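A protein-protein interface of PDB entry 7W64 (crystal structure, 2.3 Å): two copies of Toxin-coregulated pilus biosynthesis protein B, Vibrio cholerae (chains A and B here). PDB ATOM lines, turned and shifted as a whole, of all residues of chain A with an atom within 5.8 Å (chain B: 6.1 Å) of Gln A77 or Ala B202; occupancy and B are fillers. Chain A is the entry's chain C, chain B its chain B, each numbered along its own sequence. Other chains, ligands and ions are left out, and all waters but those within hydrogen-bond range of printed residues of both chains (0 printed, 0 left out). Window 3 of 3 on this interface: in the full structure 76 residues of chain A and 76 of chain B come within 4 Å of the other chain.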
ATOM      1  N   GLN A  20       6.566   8.351  15.199  1.00  0.00           N
ATOM      2  CA  GLN A  20       6.547   9.759  14.806  1.00  0.00           C
ATOM      3  C   GLN A  20       6.589   9.934  13.284  1.00  0.00           C
ATOM      4  O   GLN A  20       5.989  10.880  12.745  1.00  0.00           O
ATOM      5  CB  GLN A  20       7.689  10.509  15.491  1.00  0.00           C
ATOM      6  CG  GLN A  20       7.547  10.565  17.016  1.00  0.00           C
ATOM      7  CD  GLN A  20       6.369  11.414  17.521  1.00  0.00           C
ATOM      8  OE1 GLN A  20       5.755  12.191  16.775  1.00  0.00           O
ATOM      9  NE2 GLN A  20       6.051  11.258  18.803  1.00  0.00           N
ATOM     10  N   ARG A  23       3.106   9.460  12.083  1.00  0.00           N
ATOM     11  CA  ARG A  23       2.272  10.621  12.342  1.00  0.00           C
ATOM     12  C   ARG A  23       2.469  11.670  11.254  1.00  0.00           C
ATOM     13  O   ARG A  23       1.533  12.023  10.532  1.00  0.00           O
ATOM     14  CB  ARG A  23       2.626  11.172  13.722  1.00  0.00           C
ATOM     15  CG  ARG A  23       1.665  12.172  14.234  1.00  0.00           C
ATOM     16  CD  ARG A  23       1.803  12.349  15.723  1.00  0.00           C
ATOM     17  NE  ARG A  23       2.979  13.123  16.061  1.00  0.00           N
ATOM     18  CZ  ARG A  23       2.996  14.446  16.181  1.00  0.00           C
ATOM     19  NH1 ARG A  23       1.898  15.135  15.988  1.00  0.00           N
ATOM     20  NH2 ARG A  23       4.118  15.081  16.493  1.00  0.00           N
ATOM     21  N   ASN A  31       1.287  22.523  11.325  1.00  0.00           N
ATOM     22  CA  ASN A  31       1.346  23.917  11.768  1.00  0.00           C
ATOM     23  C   ASN A  31       0.817  24.870  10.687  1.00  0.00           C
ATOM     24  O   ASN A  31       1.435  25.893  10.380  1.00  0.00           O
ATOM     25  CB  ASN A  31       2.781  24.299  12.150  1.00  0.00           C
ATOM     26  CG  ASN A  31       3.321  23.494  13.310  1.00  0.00           C
ATOM     27  OD1 ASN A  31       2.620  23.186  14.267  1.00  0.00           O
ATOM     28  ND2 ASN A  31       4.590  23.136  13.215  1.00  0.00           N
ATOM     29  N   LEU A  56      11.935  20.636  13.416  1.00  0.00           N
ATOM     30  CA  LEU A  56      11.331  21.930  13.137  1.00  0.00           C
ATOM     31  C   LEU A  56      12.316  22.875  12.454  1.00  0.00           C
ATOM     32  O   LEU A  56      13.521  22.846  12.718  1.00  0.00           O
ATOM     33  CB  LEU A  56      10.824  22.562  14.431  1.00  0.00           C
ATOM     34  CG  LEU A  56       9.588  21.911  15.031  1.00  0.00           C
ATOM     35  CD1 LEU A  56       9.150  22.715  16.220  1.00  0.00           C
ATOM     36  CD2 LEU A  56       8.487  21.879  13.963  1.00  0.00           C
ATOM     37  N   GLN A  75       3.929  24.981  18.680  1.00  0.00           N
ATOM     38  CA  GLN A  75       4.411  24.332  17.468  1.00  0.00           C
ATOM     39  C   GLN A  75       4.276  22.823  17.623  1.00  0.00           C
ATOM     40  O   GLN A  75       4.929  22.220  18.483  1.00  0.00           O
ATOM     41  CB  GLN A  75       5.865  24.706  17.165  1.00  0.00           C
ATOM     42  CG  GLN A  75       6.125  26.191  16.890  1.00  0.00           C
ATOM     43  CD  GLN A  75       5.394  26.696  15.651  1.00  0.00           C
ATOM     44  OE1 GLN A  75       5.088  25.923  14.741  1.00  0.00           O
ATOM     45  NE2 GLN A  75       5.153  28.004  15.592  1.00  0.00           N
ATOM     46  N   ASP A  76       3.444  22.219  16.781  1.00  0.00           N
ATOM     47  CA  ASP A  76       3.425  20.770  16.670  1.00  0.00           C
ATOM     48  C   ASP A  76       4.813  20.330  16.214  1.00  0.00           C
ATOM     49  O   ASP A  76       5.412  20.952  15.330  1.00  0.00           O
ATOM     50  CB  ASP A  76       2.342  20.324  15.679  1.00  0.00           C
ATOM     51  CG  ASP A  76       1.932  18.868  15.860  1.00  0.00           C
ATOM     52  OD1 ASP A  76       2.268  18.278  16.900  1.00  0.00           O
ATOM     53  OD2 ASP A  76       1.270  18.303  14.964  1.00  0.00           O
ATOM     54  N   GLN A  77       5.363  19.317  16.875  1.00  0.00           N
ATOM     55  CA  GLN A  77       6.679  18.810  16.544  1.00  0.00           C
ATOM     56  C   GLN A  77       6.653  17.296  16.665  1.00  0.00           C
ATOM     57  O   GLN A  77       5.698  16.712  17.196  1.00  0.00           O
ATOM     58  CB  GLN A  77       7.753  19.428  17.438  1.00  0.00           C
ATOM     59  CG  GLN A  77       7.742  18.917  18.840  1.00  0.00           C
ATOM     60  CD  GLN A  77       8.813  19.557  19.661  1.00  0.00           C
ATOM     61  OE1 GLN A  77       9.201  20.693  19.398  1.00  0.00           O
ATOM     62  NE2 GLN A  77       9.325  18.829  20.654  1.00  0.00           N
ATOM     63  N   PHE A  78       7.691  16.661  16.113  1.00  0.00           N
ATOM     64  CA  PHE A  78       7.803  15.209  16.064  1.00  0.00           C
ATOM     65  C   PHE A  78       8.923  14.651  16.930  1.00  0.00           C
ATOM     66  O   PHE A  78       8.677  13.762  17.746  1.00  0.00           O
ATOM     67  CB  PHE A  78       8.002  14.777  14.606  1.00  0.00           C
ATOM     68  CG  PHE A  78       6.907  15.251  13.682  1.00  0.00           C
ATOM     69  CD1 PHE A  78       5.709  14.546  13.579  1.00  0.00           C
ATOM     70  CD2 PHE A  78       7.061  16.420  12.942  1.00  0.00           C
ATOM     71  CE1 PHE A  78       4.707  14.972  12.735  1.00  0.00           C
ATOM     72  CE2 PHE A  78       6.064  16.863  12.097  1.00  0.00           C
ATOM     73  CZ  PHE A  78       4.879  16.145  11.995  1.00  0.00           C
ATOM     74  N   ILE A  79      10.151  15.156  16.787  1.00  0.00           N
ATOM     75  CA  ILE A  79      11.284  14.743  17.607  1.00  0.00           C
ATOM     76  C   ILE A  79      11.998  15.996  18.088  1.00  0.00           C
ATOM     77  O   ILE A  79      11.853  17.081  17.516  1.00  0.00           O
ATOM     78  CB  ILE A  79      12.283  13.828  16.857  1.00  0.00           C
ATOM     79  CG1 ILE A  79      12.861  14.565  15.652  1.00  0.00           C
ATOM     80  CG2 ILE A  79      11.614  12.536  16.408  1.00  0.00           C
ATOM     81  CD1 ILE A  79      13.520  13.659  14.638  1.00  0.00           C
ATOM     82  N   ALA A  80      12.753  15.841  19.173  1.00  0.00           N
ATOM     83  CA  ALA A  80      13.543  16.970  19.628  1.00  0.00           C
ATOM     84  C   ALA A  80      14.608  17.302  18.590  1.00  0.00           C
ATOM     85  O   ALA A  80      15.022  16.462  17.788  1.00  0.00           O
ATOM     86  CB  ALA A  80      14.202  16.670  20.976  1.00  0.00           C
ATOM     87  N   LYS B 115       2.437  24.850  26.260  1.00  0.00           N
ATOM     88  CA  LYS B 115       3.385  24.487  25.210  1.00  0.00           C
ATOM     89  C   LYS B 115       4.322  23.374  25.656  1.00  0.00           C
ATOM     90  O   LYS B 115       4.458  22.374  24.945  1.00  0.00           O
ATOM     91  CB  LYS B 115       4.242  25.674  24.745  1.00  0.00           C
ATOM     92  CG  LYS B 115       3.512  26.841  24.107  1.00  0.00           C
ATOM     93  CD  LYS B 115       4.499  27.679  23.283  1.00  0.00           C
ATOM     94  CE  LYS B 115       5.600  28.299  24.112  1.00  0.00           C
ATOM     95  NZ  LYS B 115       5.086  29.253  25.118  1.00  0.00           N
ATOM     96  N   GLN B 116       4.917  23.502  26.848  1.00  0.00           N
ATOM     97  CA  GLN B 116       5.871  22.516  27.356  1.00  0.00           C
ATOM     98  C   GLN B 116       5.915  22.573  28.869  1.00  0.00           C
ATOM     99  O   GLN B 116       5.649  23.612  29.479  1.00  0.00           O
ATOM    100  CB  GLN B 116       7.303  22.695  26.827  1.00  0.00           C
ATOM    101  CG  GLN B 116       7.967  24.039  27.123  1.00  0.00           C
ATOM    102  CD  GLN B 116       9.490  24.021  26.913  1.00  0.00           C
ATOM    103  OE1 GLN B 116      10.085  22.972  26.637  1.00  0.00           O
ATOM    104  NE2 GLN B 116      10.107  25.196  26.982  1.00  0.00           N
ATOM    105  N   VAL B 117       6.247  21.433  29.458  1.00  0.00           N
ATOM    106  CA  VAL B 117       6.497  21.312  30.887  1.00  0.00           C
ATOM    107  C   VAL B 117       7.938  20.848  31.068  1.00  0.00           C
ATOM    108  O   VAL B 117       8.359  19.859  30.455  1.00  0.00           O
ATOM    109  CB  VAL B 117       5.534  20.309  31.550  1.00  0.00           C
ATOM    110  CG1 VAL B 117       5.511  20.484  33.071  1.00  0.00           C
ATOM    111  CG2 VAL B 117       4.118  20.426  30.963  1.00  0.00           C
ATOM    112  N   GLN B 150      10.190  14.169  25.984  1.00  0.00           N
ATOM    113  CA  GLN B 150      10.721  14.672  24.729  1.00  0.00           C
ATOM    114  C   GLN B 150      12.156  15.180  24.846  1.00  0.00           C
ATOM    115  O   GLN B 150      12.811  15.372  23.817  1.00  0.00           O
ATOM    116  CB  GLN B 150       9.813  15.773  24.159  1.00  0.00           C
ATOM    117  CG  GLN B 150       8.524  15.220  23.501  1.00  0.00           C
ATOM    118  CD  GLN B 150       7.613  14.491  24.474  1.00  0.00           C
ATOM    119  OE1 GLN B 150       7.053  15.092  25.386  1.00  0.00           O
ATOM    120  NE2 GLN B 150       7.528  13.174  24.328  1.00  0.00           N
ATOM    121  N   SER B 200      11.625  17.053  30.070  1.00  0.00           N
ATOM    122  CA  SER B 200      10.869  17.973  29.223  1.00  0.00           C
ATOM    123  C   SER B 200       9.742  17.282  28.466  1.00  0.00           C
ATOM    124  O   SER B 200       9.962  16.297  27.747  1.00  0.00           O
ATOM    125  CB  SER B 200      11.772  18.698  28.222  1.00  0.00           C
ATOM    126  OG  SER B 200      12.399  19.811  28.820  1.00  0.00           O
ATOM    127  N   LEU B 201       8.531  17.736  28.741  1.00  0.00           N
ATOM    128  CA  LEU B 201       7.332  17.332  28.018  1.00  0.00           C
ATOM    129  C   LEU B 201       6.999  18.419  27.006  1.00  0.00           C
ATOM    130  O   LEU B 201       6.934  19.602  27.359  1.00  0.00           O
ATOM    131  CB  LEU B 201       6.164  17.151  28.980  1.00  0.00           C
ATOM    132  CG  LEU B 201       6.395  16.044  29.987  1.00  0.00           C
ATOM    133  CD1 LEU B 201       5.201  15.939  30.914  1.00  0.00           C
ATOM    134  CD2 LEU B 201       6.605  14.763  29.210  1.00  0.00           C
ATOM    135  N   ALA B 202       6.727  18.029  25.770  1.00  0.00           N
ATOM    136  CA  ALA B 202       6.256  18.980  24.781  1.00  0.00           C
ATOM    137  C   ALA B 202       4.859  18.562  24.362  1.00  0.00           C
ATOM    138  O   ALA B 202       4.638  17.396  24.017  1.00  0.00           O
ATOM    139  CB  ALA B 202       7.185  19.050  23.571  1.00  0.00           C
ATOM    140  N   GLN B 203       3.919  19.509  24.442  1.00  0.00           N
ATOM    141  CA  GLN B 203       2.532  19.277  24.065  1.00  0.00           C
ATOM    142  C   GLN B 203       2.436  19.413  22.556  1.00  0.00           C
ATOM    143  O   GLN B 203       2.616  20.498  22.005  1.00  0.00           O
ATOM    144  CB  GLN B 203       1.658  20.284  24.790  1.00  0.00           C
ATOM    145  CG  GLN B 203       1.628  20.080  26.287  1.00  0.00           C
ATOM    146  CD  GLN B 203       0.548  19.088  26.693  1.00  0.00           C
ATOM    147  OE1 GLN B 203      -0.662  19.402  26.606  1.00  0.00           O
ATOM    148  NE2 GLN B 203       0.958  17.893  27.136  1.00  0.00           N
ATOM    149  N   THR B 204       2.155  18.316  21.883  1.00  0.00           N
ATOM    150  CA  THR B 204       2.115  18.321  20.442  1.00  0.00           C
ATOM    151  C   THR B 204       0.703  18.010  19.941  1.00  0.00           C
ATOM    152  O   THR B 204      -0.271  18.090  20.699  1.00  0.00           O
ATOM    153  CB  THR B 204       3.118  17.287  19.955  1.00  0.00           C
ATOM    154  OG1 THR B 204       2.697  16.018  20.462  1.00  0.00           O
ATOM    155  CG2 THR B 204       4.547  17.603  20.483  1.00  0.00           C
ATOM    156  N   GLY B 205       0.621  17.580  18.683  1.00  0.00           N
ATOM    157  CA  GLY B 205      -0.581  17.057  18.082  1.00  0.00           C
ATOM    158  C   GLY B 205      -0.929  15.654  18.521  1.00  0.00           C
ATOM    159  O   GLY B 205      -2.028  15.183  18.197  1.00  0.00           O
ATOM    160  N   GLU B 206      -0.043  14.988  19.272  1.00  0.00           N
ATOM    161  CA  GLU B 206      -0.324  13.637  19.742  1.00  0.00           C
ATOM    162  C   GLU B 206      -1.386  13.612  20.823  1.00  0.00           C
ATOM    163  O   GLU B 206      -1.968  12.545  21.055  1.00  0.00           O
ATOM    164  CB  GLU B 206       0.932  12.946  20.300  1.00  0.00           C
ATOM    165  CG  GLU B 206       1.885  12.356  19.295  1.00  0.00           C
ATOM    166  CD  GLU B 206       3.017  11.573  19.975  1.00  0.00           C
ATOM    167  OE1 GLU B 206       2.863  10.361  20.295  1.00  0.00           O
ATOM    168  OE2 GLU B 206       4.073  12.202  20.212  1.00  0.00           O
ATOM    169  N   ILE B 207      -1.615  14.735  21.509  1.00  0.00           N
ATOM    170  CA  ILE B 207      -2.564  14.786  22.617  1.00  0.00           C
ATOM    171  C   ILE B 207      -3.848  14.076  22.231  1.00  0.00           C
ATOM    172  O   ILE B 207      -4.380  14.293  21.138  1.00  0.00           O
ATOM    173  CB  ILE B 207      -2.820  16.246  23.012  1.00  0.00           C
ATOM    174  CG1 ILE B 207      -1.528  16.841  23.565  1.00  0.00           C
ATOM    175  CG2 ILE B 207      -3.956  16.340  23.995  1.00  0.00           C
ATOM    176  CD1 ILE B 207      -1.097  16.183  24.851  1.00  0.00           C
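No position is printed for both chains.
Printed residues of chain B within 4 Å of Gln A77: Ala B202 (3.6 Å) and Thr B204 (3.6 Å).
Ala B202 touches just one residue of chain A: Gln A77.
Printed residues of chain B within 4 Å of Arg A23: Gly B205 and Glu B206.
Of the printed residues of chain B, Ala A80 touches Gln B150.
Of the printed residues of chain B, Gln A20 touches Glu B206 (2.6 Å).
Of the printed residues of chain B, Asp A76 touches Thr B204 and Gly B205.
Of the printed residues of chain A, Gln B150 touches Ala A80 (3.4 Å).
Leu A56 touches none of the printed residues of chain B.
Val B117 touches none of the printed residues of chain A.
The nearest residue of chain B that does not touch Gln A77 is Gln B150 (4.7 Å).
The nearest printed residue of chain A that does not touch Ala B202 is Gln A75 (6.4 Å).
The nearest printed residue of chain B that does not touch Gln A20 is Gln B150 (6.0 Å).
Printed residues of chain B that touch a printed residue of chain A: Gln B150, Ala B202, Thr B204, Gly B205 and Glu B206.
Hydrophobic or aromatic side chains of chain B within 4 Å of the printed part of chain A: Ala B202.
Of the 10 printed residues of chain A, 5 touch a printed residue of chain B.
Among the printed residues, 8 pairs touch across the chains.
Gly B205 touches Arg A23.
CG of Glu B206 touches NE of Arg A23, at 3.5 Å.
Thr B204 touches Asp A76.
CB of Ala B202 touches NE2 of Gln A77, at 3.6 Å.
O of Gln A77 touches CG2 of Thr B204 (3.6 Å).
Gln B150 touches Ala A80 (O to CB, 3.4 Å).
The side-chain amide nitrogen (NE2) of Gln A20 is in hydrogen-bond range of the side-chain carboxylate (OE2) of Glu B206, at 2.6 Å.
N of Gly B205 lies within hydrogen-bond range of OD1 of Asp A76 (2.5 Å).
The side-chain amide oxygen of Gln A20 is in hydrogen-bond range of the guanidinium group of Arg A23, 3.0 Å away.
The side-chain amide oxygen (OD1) of Asn A31 lies within hydrogen-bond range of the backbone NH (N) of Asp A76 (2.8 Å).
OG1 of Thr B204 is in hydrogen-bond range of N of Glu B206, at 3.2 Å.
The backbone NH (N) of Ala B202 lies within hydrogen-bond range of the side-chain amide oxygen (OE1) of Gln B150 (3.0 Å).
OE1 of Gln A20 lies close to O of Phe A78 (3.5 Å).
O of Ser B200 lies within hydrogen-bond range of N of Gln B150, 2.8 Å away.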
